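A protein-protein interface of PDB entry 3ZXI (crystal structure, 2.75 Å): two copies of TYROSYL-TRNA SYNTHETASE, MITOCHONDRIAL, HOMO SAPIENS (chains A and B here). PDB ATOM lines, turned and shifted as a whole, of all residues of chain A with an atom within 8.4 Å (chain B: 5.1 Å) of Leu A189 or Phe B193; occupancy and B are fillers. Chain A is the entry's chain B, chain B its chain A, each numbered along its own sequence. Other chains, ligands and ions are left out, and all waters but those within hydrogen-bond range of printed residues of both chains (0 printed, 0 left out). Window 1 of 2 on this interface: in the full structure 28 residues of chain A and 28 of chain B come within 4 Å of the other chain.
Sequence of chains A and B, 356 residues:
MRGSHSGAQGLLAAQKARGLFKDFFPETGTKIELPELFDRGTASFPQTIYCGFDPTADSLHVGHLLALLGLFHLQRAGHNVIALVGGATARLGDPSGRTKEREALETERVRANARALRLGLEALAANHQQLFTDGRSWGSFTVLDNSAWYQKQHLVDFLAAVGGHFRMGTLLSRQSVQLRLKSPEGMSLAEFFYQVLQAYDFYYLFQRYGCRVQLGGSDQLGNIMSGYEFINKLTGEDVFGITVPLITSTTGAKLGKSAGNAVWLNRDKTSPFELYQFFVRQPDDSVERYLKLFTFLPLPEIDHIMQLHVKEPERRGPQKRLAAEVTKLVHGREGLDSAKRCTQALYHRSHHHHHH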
ATOM      1  N   LEU A  92     -14.212 -22.947  17.811  1.00  0.00           N
ATOM      2  CA  LEU A  92     -14.784 -23.931  18.718  1.00  0.00           C
ATOM      3  C   LEU A  92     -16.205 -24.294  18.297  1.00  0.00           C
ATOM      4  O   LEU A  92     -16.492 -25.437  17.923  1.00  0.00           O
ATOM      5  CB  LEU A  92     -14.818 -23.363  20.135  1.00  0.00           C
ATOM      6  CG  LEU A  92     -13.666 -23.694  21.070  1.00  0.00           C
ATOM      7  CD1 LEU A  92     -12.315 -23.498  20.377  1.00  0.00           C
ATOM      8  CD2 LEU A  92     -13.779 -22.855  22.334  1.00  0.00           C
ATOM      9  N   PRO A  95     -22.148 -24.597  21.678  1.00  0.00           N
ATOM     10  CA  PRO A  95     -22.924 -25.794  21.981  1.00  0.00           C
ATOM     11  C   PRO A  95     -24.416 -25.471  22.171  1.00  0.00           C
ATOM     12  O   PRO A  95     -25.277 -26.322  21.914  1.00  0.00           O
ATOM     13  CB  PRO A  95     -22.309 -26.252  23.306  1.00  0.00           C
ATOM     14  CG  PRO A  95     -21.847 -24.982  23.946  1.00  0.00           C
ATOM     15  CD  PRO A  95     -21.298 -24.189  22.813  1.00  0.00           C
ATOM     16  N   GLU A 101     -22.583 -32.535  18.028  1.00  0.00           N
ATOM     17  CA  GLU A 101     -21.278 -31.890  17.956  1.00  0.00           C
ATOM     18  C   GLU A 101     -21.044 -31.333  16.553  1.00  0.00           C
ATOM     19  O   GLU A 101     -21.418 -31.962  15.562  1.00  0.00           O
ATOM     20  CB  GLU A 101     -20.169 -32.873  18.351  1.00  0.00           C
ATOM     21  CG  GLU A 101     -18.760 -32.297  18.279  1.00  0.00           C
ATOM     22  CD  GLU A 101     -17.836 -32.867  19.340  1.00  0.00           C
ATOM     23  OE1 GLU A 101     -18.348 -33.397  20.350  1.00  0.00           O
ATOM     24  OE2 GLU A 101     -16.601 -32.776  19.164  1.00  0.00           O
ATOM     25  N   LEU A 155      -2.858 -19.993  27.080  1.00  0.00           N
ATOM     26  CA  LEU A 155      -3.549 -20.994  27.883  1.00  0.00           C
ATOM     27  C   LEU A 155      -3.384 -20.899  29.410  1.00  0.00           C
ATOM     28  O   LEU A 155      -4.336 -20.497  30.100  1.00  0.00           O
ATOM     29  CB  LEU A 155      -3.161 -22.387  27.412  1.00  0.00           C
ATOM     30  CG  LEU A 155      -3.907 -23.495  28.153  1.00  0.00           C
ATOM     31  CD1 LEU A 155      -4.732 -24.322  27.203  1.00  0.00           C
ATOM     32  CD2 LEU A 155      -2.910 -24.360  28.864  1.00  0.00           C
ATOM     33  N   VAL A 156      -2.209 -21.289  29.929  1.00  0.00           N
ATOM     34  CA  VAL A 156      -1.957 -21.266  31.372  1.00  0.00           C
ATOM     35  C   VAL A 156      -2.097 -19.880  32.018  1.00  0.00           C
ATOM     36  O   VAL A 156      -2.460 -19.770  33.192  1.00  0.00           O
ATOM     37  CB  VAL A 156      -0.601 -21.933  31.763  1.00  0.00           C
ATOM     38  CG1 VAL A 156      -0.402 -21.978  33.292  1.00  0.00           C
ATOM     39  CG2 VAL A 156      -0.535 -23.333  31.235  1.00  0.00           C
ATOM     40  N   LEU A 159      -5.961 -19.503  32.311  1.00  0.00           N
ATOM     41  CA  LEU A 159      -6.332 -20.398  33.387  1.00  0.00           C
ATOM     42  C   LEU A 159      -5.867 -19.907  34.739  1.00  0.00           C
ATOM     43  O   LEU A 159      -6.586 -20.001  35.739  1.00  0.00           O
ATOM     44  CB  LEU A 159      -5.761 -21.784  33.126  1.00  0.00           C
ATOM     45  CG  LEU A 159      -6.372 -22.522  31.941  1.00  0.00           C
ATOM     46  CD1 LEU A 159      -5.683 -23.866  31.748  1.00  0.00           C
ATOM     47  CD2 LEU A 159      -7.846 -22.696  32.181  1.00  0.00           C
ATOM     48  N   GLY A 163      -9.419 -18.928  35.672  1.00  0.00           N
ATOM     49  CA  GLY A 163      -9.918 -20.269  35.914  1.00  0.00           C
ATOM     50  C   GLY A 163     -10.335 -20.539  37.348  1.00  0.00           C
ATOM     51  O   GLY A 163     -11.216 -21.362  37.605  1.00  0.00           O
ATOM     52  N   MET A 168     -16.920 -24.912  39.021  1.00  0.00           N
ATOM     53  CA  MET A 168     -17.326 -25.965  38.095  1.00  0.00           C
ATOM     54  C   MET A 168     -18.832 -26.263  38.152  1.00  0.00           C
ATOM     55  O   MET A 168     -19.459 -26.507  37.122  1.00  0.00           O
ATOM     56  CB  MET A 168     -16.504 -27.239  38.307  1.00  0.00           C
ATOM     57  CG  MET A 168     -15.203 -27.257  37.532  1.00  0.00           C
ATOM     58  SD  MET A 168     -15.524 -27.088  35.764  1.00  0.00           S
ATOM     59  CE  MET A 168     -15.614 -28.785  35.210  1.00  0.00           C
ATOM     60  N   GLY A 186     -21.590 -37.421  24.938  1.00  0.00           N
ATOM     61  CA  GLY A 186     -20.990 -36.453  25.834  1.00  0.00           C
ATOM     62  C   GLY A 186     -20.550 -35.228  25.065  1.00  0.00           C
ATOM     63  O   GLY A 186     -20.713 -35.140  23.848  1.00  0.00           O
ATOM     64  N   MET A 187     -19.987 -34.266  25.777  1.00  0.00           N
ATOM     65  CA  MET A 187     -19.586 -33.037  25.135  1.00  0.00           C
ATOM     66  C   MET A 187     -18.075 -32.856  25.199  1.00  0.00           C
ATOM     67  O   MET A 187     -17.446 -33.116  26.234  1.00  0.00           O
ATOM     68  CB  MET A 187     -20.298 -31.863  25.777  1.00  0.00           C
ATOM     69  CG  MET A 187     -19.865 -31.538  27.193  1.00  0.00           C
ATOM     70  SD  MET A 187     -20.522 -29.916  27.713  1.00  0.00           S
ATOM     71  CE  MET A 187     -20.996 -29.184  26.141  1.00  0.00           C
ATOM     72  N   SER A 188     -17.488 -32.427  24.087  1.00  0.00           N
ATOM     73  CA  SER A 188     -16.052 -32.227  24.057  1.00  0.00           C
ATOM     74  C   SER A 188     -15.720 -31.230  25.139  1.00  0.00           C
ATOM     75  O   SER A 188     -16.596 -30.488  25.593  1.00  0.00           O
ATOM     76  CB  SER A 188     -15.606 -31.673  22.710  1.00  0.00           C
ATOM     77  OG  SER A 188     -15.979 -30.309  22.591  1.00  0.00           O
ATOM     78  N   LEU A 189     -14.459 -31.239  25.553  1.00  0.00           N
ATOM     79  CA  LEU A 189     -13.898 -30.201  26.400  1.00  0.00           C
ATOM     80  C   LEU A 189     -14.125 -28.823  25.800  1.00  0.00           C
ATOM     81  O   LEU A 189     -14.442 -27.895  26.520  1.00  0.00           O
ATOM     82  CB  LEU A 189     -12.396 -30.424  26.555  1.00  0.00           C
ATOM     83  CG  LEU A 189     -11.672 -29.414  27.427  1.00  0.00           C
ATOM     84  CD1 LEU A 189     -12.082 -29.531  28.908  1.00  0.00           C
ATOM     85  CD2 LEU A 189     -10.204 -29.638  27.256  1.00  0.00           C
ATOM     86  N   ALA A 190     -13.936 -28.714  24.483  1.00  0.00           N
ATOM     87  CA  ALA A 190     -14.049 -27.448  23.749  1.00  0.00           C
ATOM     88  C   ALA A 190     -15.441 -26.849  23.877  1.00  0.00           C
ATOM     89  O   ALA A 190     -15.597 -25.685  24.243  1.00  0.00           O
ATOM     90  CB  ALA A 190     -13.697 -27.648  22.262  1.00  0.00           C
ATOM     91  N   GLU A 191     -16.448 -27.659  23.568  1.00  0.00           N
ATOM     92  CA  GLU A 191     -17.840 -27.245  23.673  1.00  0.00           C
ATOM     93  C   GLU A 191     -18.126 -26.658  25.035  1.00  0.00           C
ATOM     94  O   GLU A 191     -18.744 -25.601  25.165  1.00  0.00           O
ATOM     95  CB  GLU A 191     -18.770 -28.440  23.478  1.00  0.00           C
ATOM     96  CG  GLU A 191     -18.884 -28.924  22.056  1.00  0.00           C
ATOM     97  CD  GLU A 191     -19.786 -30.132  21.936  1.00  0.00           C
ATOM     98  OE1 GLU A 191     -19.656 -31.058  22.770  1.00  0.00           O
ATOM     99  OE2 GLU A 191     -20.621 -30.161  21.009  1.00  0.00           O
ATOM    100  N   PHE A 192     -17.696 -27.375  26.055  1.00  0.00           N
ATOM    101  CA  PHE A 192     -17.919 -26.952  27.417  1.00  0.00           C
ATOM    102  C   PHE A 192     -17.183 -25.644  27.704  1.00  0.00           C
ATOM    103  O   PHE A 192     -17.692 -24.797  28.457  1.00  0.00           O
ATOM    104  CB  PHE A 192     -17.426 -28.031  28.363  1.00  0.00           C
ATOM    105  CG  PHE A 192     -17.248 -27.564  29.765  1.00  0.00           C
ATOM    106  CD1 PHE A 192     -18.315 -27.546  30.633  1.00  0.00           C
ATOM    107  CD2 PHE A 192     -16.012 -27.138  30.223  1.00  0.00           C
ATOM    108  CE1 PHE A 192     -18.155 -27.124  31.942  1.00  0.00           C
ATOM    109  CE2 PHE A 192     -15.850 -26.702  31.531  1.00  0.00           C
ATOM    110  CZ  PHE A 192     -16.924 -26.702  32.391  1.00  0.00           C
ATOM    111  N   PHE A 193     -15.987 -25.481  27.122  1.00  0.00           N
ATOM    112  CA  PHE A 193     -15.137 -24.349  27.485  1.00  0.00           C
ATOM    113  C   PHE A 193     -15.662 -23.086  26.829  1.00  0.00           C
ATOM    114  O   PHE A 193     -15.452 -21.978  27.324  1.00  0.00           O
ATOM    115  CB  PHE A 193     -13.671 -24.571  27.130  1.00  0.00           C
ATOM    116  CG  PHE A 193     -12.735 -23.691  27.912  1.00  0.00           C
ATOM    117  CD1 PHE A 193     -12.472 -22.398  27.499  1.00  0.00           C
ATOM    118  CD2 PHE A 193     -12.147 -24.147  29.084  1.00  0.00           C
ATOM    119  CE1 PHE A 193     -11.623 -21.580  28.227  1.00  0.00           C
ATOM    120  CE2 PHE A 193     -11.297 -23.337  29.821  1.00  0.00           C
ATOM    121  CZ  PHE A 193     -11.031 -22.054  29.392  1.00  0.00           C
ATOM    122  N   TYR A 194     -16.380 -23.290  25.732  1.00  0.00           N
ATOM    123  CA  TYR A 194     -16.993 -22.216  24.967  1.00  0.00           C
ATOM    124  C   TYR A 194     -17.649 -21.144  25.821  1.00  0.00           C
ATOM    125  O   TYR A 194     -17.376 -19.957  25.645  1.00  0.00           O
ATOM    126  CB  TYR A 194     -18.027 -22.779  24.016  1.00  0.00           C
ATOM    127  CG  TYR A 194     -18.503 -21.761  23.017  1.00  0.00           C
ATOM    128  CD1 TYR A 194     -19.456 -20.799  23.364  1.00  0.00           C
ATOM    129  CD2 TYR A 194     -18.006 -21.759  21.721  1.00  0.00           C
ATOM    130  CE1 TYR A 194     -19.902 -19.871  22.442  1.00  0.00           C
ATOM    131  CE2 TYR A 194     -18.438 -20.824  20.786  1.00  0.00           C
ATOM    132  CZ  TYR A 194     -19.381 -19.878  21.151  1.00  0.00           C
ATOM    133  OH  TYR A 194     -19.804 -18.945  20.216  1.00  0.00           O
ATOM    134  N   GLN A 195     -18.529 -21.550  26.728  1.00  0.00           N
ATOM    135  CA  GLN A 195     -19.210 -20.578  27.580  1.00  0.00           C
ATOM    136  C   GLN A 195     -18.214 -19.702  28.313  1.00  0.00           C
ATOM    137  O   GLN A 195     -18.473 -18.531  28.562  1.00  0.00           O
ATOM    138  CB  GLN A 195     -20.113 -21.267  28.605  1.00  0.00           C
ATOM    139  CG  GLN A 195     -19.834 -22.742  28.771  1.00  0.00           C
ATOM    140  CD  GLN A 195     -20.474 -23.284  30.015  1.00  0.00           C
ATOM    141  OE1 GLN A 195     -20.741 -22.540  30.965  1.00  0.00           O
ATOM    142  NE2 GLN A 195     -20.736 -24.585  30.024  1.00  0.00           N
ATOM    143  N   VAL A 196     -17.073 -20.273  28.671  1.00  0.00           N
ATOM    144  CA  VAL A 196     -16.080 -19.524  29.442  1.00  0.00           C
ATOM    145  C   VAL A 196     -15.498 -18.327  28.683  1.00  0.00           C
ATOM    146  O   VAL A 196     -15.304 -17.262  29.258  1.00  0.00           O
ATOM    147  CB  VAL A 196     -14.982 -20.443  29.965  1.00  0.00           C
ATOM    148  CG1 VAL A 196     -13.752 -19.635  30.418  1.00  0.00           C
ATOM    149  CG2 VAL A 196     -15.549 -21.318  31.104  1.00  0.00           C
ATOM    150  N   LEU B  92      -1.317 -23.631  38.490  1.00  0.00           N
ATOM    151  CA  LEU B  92      -2.641 -24.140  38.789  1.00  0.00           C
ATOM    152  C   LEU B  92      -2.672 -24.915  40.110  1.00  0.00           C
ATOM    153  O   LEU B  92      -3.311 -24.497  41.071  1.00  0.00           O
ATOM    154  CB  LEU B  92      -3.073 -25.056  37.657  1.00  0.00           C
ATOM    155  CG  LEU B  92      -3.890 -24.450  36.516  1.00  0.00           C
ATOM    156  CD1 LEU B  92      -3.326 -23.122  36.040  1.00  0.00           C
ATOM    157  CD2 LEU B  92      -4.010 -25.464  35.378  1.00  0.00           C
ATOM    158  N   PHE B 158      -5.171 -24.256  21.558  1.00  0.00           N
ATOM    159  CA  PHE B 158      -5.255 -25.486  22.342  1.00  0.00           C
ATOM    160  C   PHE B 158      -6.669 -26.056  22.300  1.00  0.00           C
ATOM    161  O   PHE B 158      -6.866 -27.165  21.837  1.00  0.00           O
ATOM    162  CB  PHE B 158      -4.880 -25.187  23.786  1.00  0.00           C
ATOM    163  CG  PHE B 158      -4.762 -26.398  24.647  1.00  0.00           C
ATOM    164  CD1 PHE B 158      -5.863 -27.186  24.909  1.00  0.00           C
ATOM    165  CD2 PHE B 158      -3.539 -26.730  25.225  1.00  0.00           C
ATOM    166  CE1 PHE B 158      -5.753 -28.306  25.719  1.00  0.00           C
ATOM    167  CE2 PHE B 158      -3.416 -27.846  26.035  1.00  0.00           C
ATOM    168  CZ  PHE B 158      -4.526 -28.641  26.281  1.00  0.00           C
ATOM    169  N   LEU B 159      -7.639 -25.278  22.783  1.00  0.00           N
ATOM    170  CA  LEU B 159      -9.025 -25.704  22.837  1.00  0.00           C
ATOM    171  C   LEU B 159      -9.487 -26.172  21.471  1.00  0.00           C
ATOM    172  O   LEU B 159     -10.213 -27.175  21.334  1.00  0.00           O
ATOM    173  CB  LEU B 159      -9.914 -24.564  23.310  1.00  0.00           C
ATOM    174  CG  LEU B 159      -9.712 -24.219  24.773  1.00  0.00           C
ATOM    175  CD1 LEU B 159     -10.649 -23.092  25.145  1.00  0.00           C
ATOM    176  CD2 LEU B 159      -9.995 -25.471  25.589  1.00  0.00           C
ATOM    177  N   VAL B 162      -7.450 -29.634  20.534  1.00  0.00           N
ATOM    178  CA  VAL B 162      -7.560 -30.843  21.343  1.00  0.00           C
ATOM    179  C   VAL B 162      -8.883 -30.944  22.110  1.00  0.00           C
ATOM    180  O   VAL B 162      -9.428 -32.033  22.262  1.00  0.00           O
ATOM    181  CB  VAL B 162      -6.387 -30.927  22.341  1.00  0.00           C
ATOM    182  CG1 VAL B 162      -5.189 -30.161  21.795  1.00  0.00           C
ATOM    183  CG2 VAL B 162      -6.788 -30.342  23.685  1.00  0.00           C
ATOM    184  N   GLY B 163      -9.388 -29.813  22.599  1.00  0.00           N
ATOM    185  CA  GLY B 163     -10.594 -29.800  23.413  1.00  0.00           C
ATOM    186  C   GLY B 163     -11.706 -30.710  22.913  1.00  0.00           C
ATOM    187  O   GLY B 163     -12.509 -31.224  23.696  1.00  0.00           O
ATOM    188  N   GLY B 164     -11.755 -30.923  21.604  1.00  0.00           N
ATOM    189  CA  GLY B 164     -12.791 -31.753  21.027  1.00  0.00           C
ATOM    190  C   GLY B 164     -12.549 -33.233  21.211  1.00  0.00           C
ATOM    191  O   GLY B 164     -13.411 -34.032  20.839  1.00  0.00           O
ATOM    192  N   PHE B 166     -11.478 -34.543  24.313  1.00  0.00           N
ATOM    193  CA  PHE B 166     -11.695 -34.870  25.705  1.00  0.00           C
ATOM    194  C   PHE B 166     -13.180 -34.895  25.996  1.00  0.00           C
ATOM    195  O   PHE B 166     -13.783 -33.847  26.223  1.00  0.00           O
ATOM    196  CB  PHE B 166     -11.039 -33.821  26.597  1.00  0.00           C
ATOM    197  CG  PHE B 166      -9.556 -33.921  26.649  1.00  0.00           C
ATOM    198  CD1 PHE B 166      -8.816 -33.954  25.488  1.00  0.00           C
ATOM    199  CD2 PHE B 166      -8.902 -33.973  27.867  1.00  0.00           C
ATOM    200  CE1 PHE B 166      -7.450 -34.042  25.539  1.00  0.00           C
ATOM    201  CE2 PHE B 166      -7.536 -34.064  27.927  1.00  0.00           C
ATOM    202  CZ  PHE B 166      -6.804 -34.096  26.761  1.00  0.00           C
ATOM    203  N   ARG B 167     -13.779 -36.077  25.972  1.00  0.00           N
ATOM    204  CA  ARG B 167     -15.166 -36.211  26.372  1.00  0.00           C
ATOM    205  C   ARG B 167     -15.312 -35.763  27.809  1.00  0.00           C
ATOM    206  O   ARG B 167     -14.583 -36.215  28.680  1.00  0.00           O
ATOM    207  CB  ARG B 167     -15.612 -37.654  26.250  1.00  0.00           C
ATOM    208  CG  ARG B 167     -15.684 -38.157  24.835  1.00  0.00           C
ATOM    209  CD  ARG B 167     -16.842 -37.522  24.131  1.00  0.00           C
ATOM    210  NE  ARG B 167     -16.397 -36.625  23.077  1.00  0.00           N
ATOM    211  CZ  ARG B 167     -17.218 -36.018  22.230  1.00  0.00           C
ATOM    212  NH1 ARG B 167     -18.530 -36.220  22.319  1.00  0.00           N
ATOM    213  NH2 ARG B 167     -16.727 -35.221  21.290  1.00  0.00           N
ATOM    214  N   MET B 168     -16.268 -34.879  28.054  1.00  0.00           N
ATOM    215  CA  MET B 168     -16.505 -34.360  29.397  1.00  0.00           C
ATOM    216  C   MET B 168     -16.805 -35.440  30.443  1.00  0.00           C
ATOM    217  O   MET B 168     -16.354 -35.335  31.584  1.00  0.00           O
ATOM    218  CB  MET B 168     -17.610 -33.296  29.368  1.00  0.00           C
ATOM    219  CG  MET B 168     -17.103 -31.873  29.049  1.00  0.00           C
ATOM    220  SD  MET B 168     -15.828 -31.313  30.211  1.00  0.00           S
ATOM    221  CE  MET B 168     -16.834 -30.472  31.441  1.00  0.00           C
ATOM    222  N   LEU B 189     -12.562 -24.113  37.956  1.00  0.00           N
ATOM    223  CA  LEU B 189     -12.280 -24.517  36.595  1.00  0.00           C
ATOM    224  C   LEU B 189     -10.833 -24.948  36.427  1.00  0.00           C
ATOM    225  O   LEU B 189     -10.541 -25.887  35.694  1.00  0.00           O
ATOM    226  CB  LEU B 189     -12.503 -23.325  35.689  1.00  0.00           C
ATOM    227  CG  LEU B 189     -12.238 -23.570  34.219  1.00  0.00           C
ATOM    228  CD1 LEU B 189     -13.271 -24.570  33.646  1.00  0.00           C
ATOM    229  CD2 LEU B 189     -12.265 -22.197  33.505  1.00  0.00           C
ATOM    230  N   ALA B 190      -9.929 -24.220  37.081  1.00  0.00           N
ATOM    231  CA  ALA B 190      -8.499 -24.471  36.979  1.00  0.00           C
ATOM    232  C   ALA B 190      -8.142 -25.875  37.447  1.00  0.00           C
ATOM    233  O   ALA B 190      -7.438 -26.606  36.740  1.00  0.00           O
ATOM    234  CB  ALA B 190      -7.706 -23.419  37.780  1.00  0.00           C
ATOM    235  N   GLU B 191      -8.616 -26.226  38.648  1.00  0.00           N
ATOM    236  CA  GLU B 191      -8.377 -27.531  39.262  1.00  0.00           C
ATOM    237  C   GLU B 191      -8.778 -28.628  38.305  1.00  0.00           C
ATOM    238  O   GLU B 191      -8.048 -29.593  38.095  1.00  0.00           O
ATOM    239  CB  GLU B 191      -9.210 -27.678  40.526  1.00  0.00           C
ATOM    240  CG  GLU B 191      -8.704 -26.912  41.713  1.00  0.00           C
ATOM    241  CD  GLU B 191      -9.574 -27.111  42.942  1.00  0.00           C
ATOM    242  OE1 GLU B 191     -10.809 -27.014  42.813  1.00  0.00           O
ATOM    243  OE2 GLU B 191      -9.023 -27.373  44.036  1.00  0.00           O
ATOM    244  N   PHE B 192      -9.965 -28.470  37.740  1.00  0.00           N
ATOM    245  CA  PHE B 192     -10.498 -29.423  36.798  1.00  0.00           C
ATOM    246  C   PHE B 192      -9.690 -29.483  35.513  1.00  0.00           C
ATOM    247  O   PHE B 192      -9.582 -30.527  34.882  1.00  0.00           O
ATOM    248  CB  PHE B 192     -11.940 -29.061  36.467  1.00  0.00           C
ATOM    249  CG  PHE B 192     -12.483 -29.778  35.269  1.00  0.00           C
ATOM    250  CD1 PHE B 192     -13.075 -31.027  35.398  1.00  0.00           C
ATOM    251  CD2 PHE B 192     -12.413 -29.197  34.010  1.00  0.00           C
ATOM    252  CE1 PHE B 192     -13.590 -31.681  34.290  1.00  0.00           C
ATOM    253  CE2 PHE B 192     -12.924 -29.853  32.896  1.00  0.00           C
ATOM    254  CZ  PHE B 192     -13.519 -31.093  33.037  1.00  0.00           C
ATOM    255  N   PHE B 193      -9.149 -28.353  35.094  1.00  0.00           N
ATOM    256  CA  PHE B 193      -8.494 -28.324  33.795  1.00  0.00           C
ATOM    257  C   PHE B 193      -7.110 -28.922  33.901  1.00  0.00           C
ATOM    258  O   PHE B 193      -6.557 -29.406  32.916  1.00  0.00           O
ATOM    259  CB  PHE B 193      -8.425 -26.912  33.221  1.00  0.00           C
ATOM    260  CG  PHE B 193      -8.228 -26.894  31.742  1.00  0.00           C
ATOM    261  CD1 PHE B 193      -6.966 -27.025  31.197  1.00  0.00           C
ATOM    262  CD2 PHE B 193      -9.306 -26.783  30.886  1.00  0.00           C
ATOM    263  CE1 PHE B 193      -6.780 -27.021  29.822  1.00  0.00           C
ATOM    264  CE2 PHE B 193      -9.126 -26.782  29.511  1.00  0.00           C
ATOM    265  CZ  PHE B 193      -7.858 -26.901  28.982  1.00  0.00           C
ATOM    266  N   TYR B 194      -6.573 -28.883  35.117  1.00  0.00           N
ATOM    267  CA  TYR B 194      -5.283 -29.471  35.453  1.00  0.00           C
ATOM    268  C   TYR B 194      -5.037 -30.814  34.793  1.00  0.00           C
ATOM    269  O   TYR B 194      -4.016 -30.999  34.134  1.00  0.00           O
ATOM    270  CB  TYR B 194      -5.164 -29.646  36.956  1.00  0.00           C
ATOM    271  CG  TYR B 194      -3.761 -29.942  37.370  1.00  0.00           C
ATOM    272  CD1 TYR B 194      -3.225 -31.207  37.201  1.00  0.00           C
ATOM    273  CD2 TYR B 194      -2.955 -28.953  37.909  1.00  0.00           C
ATOM    274  CE1 TYR B 194      -1.914 -31.479  37.562  1.00  0.00           C
ATOM    275  CE2 TYR B 194      -1.644 -29.221  38.280  1.00  0.00           C
ATOM    276  CZ  TYR B 194      -1.126 -30.483  38.104  1.00  0.00           C
ATOM    277  OH  TYR B 194       0.180 -30.750  38.479  1.00  0.00           O
ATOM    278  N   GLN B 195      -5.955 -31.760  34.977  1.00  0.00           N
ATOM    279  CA  GLN B 195      -5.752 -33.079  34.398  1.00  0.00           C
ATOM    280  C   GLN B 195      -5.508 -33.026  32.902  1.00  0.00           C
ATOM    281  O   GLN B 195      -4.763 -33.829  32.347  1.00  0.00           O
ATOM    282  CB  GLN B 195      -6.945 -33.959  34.664  1.00  0.00           C
ATOM    283  CG  GLN B 195      -8.178 -33.220  35.065  1.00  0.00           C
ATOM    284  CD  GLN B 195      -9.406 -34.111  34.964  1.00  0.00           C
ATOM    285  OE1 GLN B 195      -9.451 -35.035  34.156  1.00  0.00           O
ATOM    286  NE2 GLN B 195     -10.403 -33.837  35.788  1.00  0.00           N
ATOM    287  N   VAL B 196      -6.160 -32.082  32.251  1.00  0.00           N
ATOM    288  CA  VAL B 196      -6.059 -31.951  30.810  1.00  0.00           C
ATOM    289  C   VAL B 196      -4.633 -31.637  30.340  1.00  0.00           C
ATOM    290  O   VAL B 196      -4.172 -32.219  29.357  1.00  0.00           O
ATOM    291  CB  VAL B 196      -7.094 -30.925  30.296  1.00  0.00           C
ATOM    292  CG1 VAL B 196      -6.780 -30.477  28.869  1.00  0.00           C
ATOM    293  CG2 VAL B 196      -8.478 -31.540  30.393  1.00  0.00           C
ATOM    294  N   LEU B 197      -3.944 -30.732  31.038  1.00  0.00           N
ATOM    295  CA  LEU B 197      -2.543 -30.426  30.736  1.00  0.00           C
ATOM    296  C   LEU B 197      -1.644 -31.672  30.865  1.00  0.00           C
ATOM    297  O   LEU B 197      -0.965 -32.062  29.908  1.00  0.00           O
ATOM    298  CB  LEU B 197      -2.029 -29.318  31.657  1.00  0.00           C
ATOM    299  CG  LEU B 197      -3.046 -28.202  31.769  1.00  0.00           C
ATOM    300  CD1 LEU B 197      -2.596 -27.134  32.753  1.00  0.00           C
ATOM    301  CD2 LEU B 197      -3.188 -27.655  30.384  1.00  0.00           C
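Among the printed residues, pairs that only touch across the chains: Phe A193 with Leu B159 (3.1 Å), Ser A188 with Gly B164 (3.3 Å), Ser A188 with Gly B163 (3.3 Å), Met A168 with Phe B192 (3.3 Å), Leu A155 with Phe B158 (3.3 Å), Phe A192 with Met B168 (3.4 Å), Ser A188 with Phe B166 (3.4 Å), Leu A159 with Phe B193 (3.5 Å), Ala A190 with Leu B159 (3.6 Å), Leu A155 with Leu B197 (3.6 Å), Met A187 with Phe B166 (3.7 Å), Met A187 with Arg B167 (3.7 Å), Ser A188 with Met B168 (3.8 Å), Leu A189 with Phe B193 (3.8 Å), Glu A101 with Gly B164 (3.8 Å), Ala A190 with Gly B164 (3.9 Å), Leu A189 with Val B196 (3.9 Å), Leu A92 with Leu B159 (3.9 Å), Phe A192 with Leu B189 (3.96 Å), Phe A193 with Leu B189 (3.98 Å), Ser A188 with Arg B167 (3.98 Å) and Met A168 with Leu B189 (3.99 Å).
The side-chain hydroxyl of Ser A188 sits close to the backbone NH of Ala A190 (3.2 Å). The side-chain hydroxyl (OG) of Ser A188 is in hydrogen-bond range of the backbone NH (N) of Glu A191, at 2.9 Å. O of Phe A192 lies close to NE2 of Gln A195 (3.4 Å).
Printed residues of chain A that touch a printed residue of chain B: Leu A92, Glu A101, Leu A155, Leu A159, Gly A163, Met A168, Gly A186, Met A187, Ser A188, Leu A189, Ala A190, Phe A192 and Phe A193. Hydrophobic or aromatic side chains of chain A that line the printed part of chain B: Leu A92, Leu A155, Leu A159, Met A168, Met A187, Leu A189, Ala A190, Phe A192 and Phe A193. Among the printed residues, 30 pairs touch across the chains. Among the printed residues, Asp or Glu carboxylates within 4 Å of a Lys or Arg side-chain nitrogen of the other chain: Glu A101 with Arg B167 (2.6 Å).
Printed residues of chain B within 4 Å of Leu A159: Phe B193. Of the printed residues of chain B, Leu A189 touches Gly B163, Phe B166, Phe B193 and Val B196. Of chain A, only Leu A159 and Leu A189 come within 4 Å of Phe B193. Of the printed residues of chain A, Leu B197 touches Leu A155.
Gly A163 touches Ala B190, and with the chains exchanged Ala A190 touches Gly B163. Leu A189 touches Phe B193, and with the chains exchanged Phe A193 touches Leu B189.
The backbone NH of Leu A189 sits at hydrogen-bond distance from the backbone carbonyl oxygen of Gly B163. N of Ala B190 sits at hydrogen-bond distance from O of Gly A163 (3.2 Å). The backbone NH (N) of Leu B189 sits close to the backbone carbonyl oxygen (O) of Gly A163, 3.1 Å away. N of Ala A190 lies within hydrogen-bond range of O of Gly B163 (3.0 Å). The backbone carbonyl oxygen (O) of Met A187 lies within hydrogen-bond range of the backbone NH (N) of Met B168, 2.8 Å away. The backbone NH (N) of Leu A189 is in hydrogen-bond range of the backbone carbonyl oxygen (O) of Phe B166. The guanidinium group (NH2) of Arg B167 lies within salt-bridge range of the side-chain carboxylate (OE1) of Glu A101. The backbone carbonyl oxygen (O) of Gly A186 is in hydrogen-bond range of the guanidinium group (NH1) of Arg B167 (2.9 Å).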
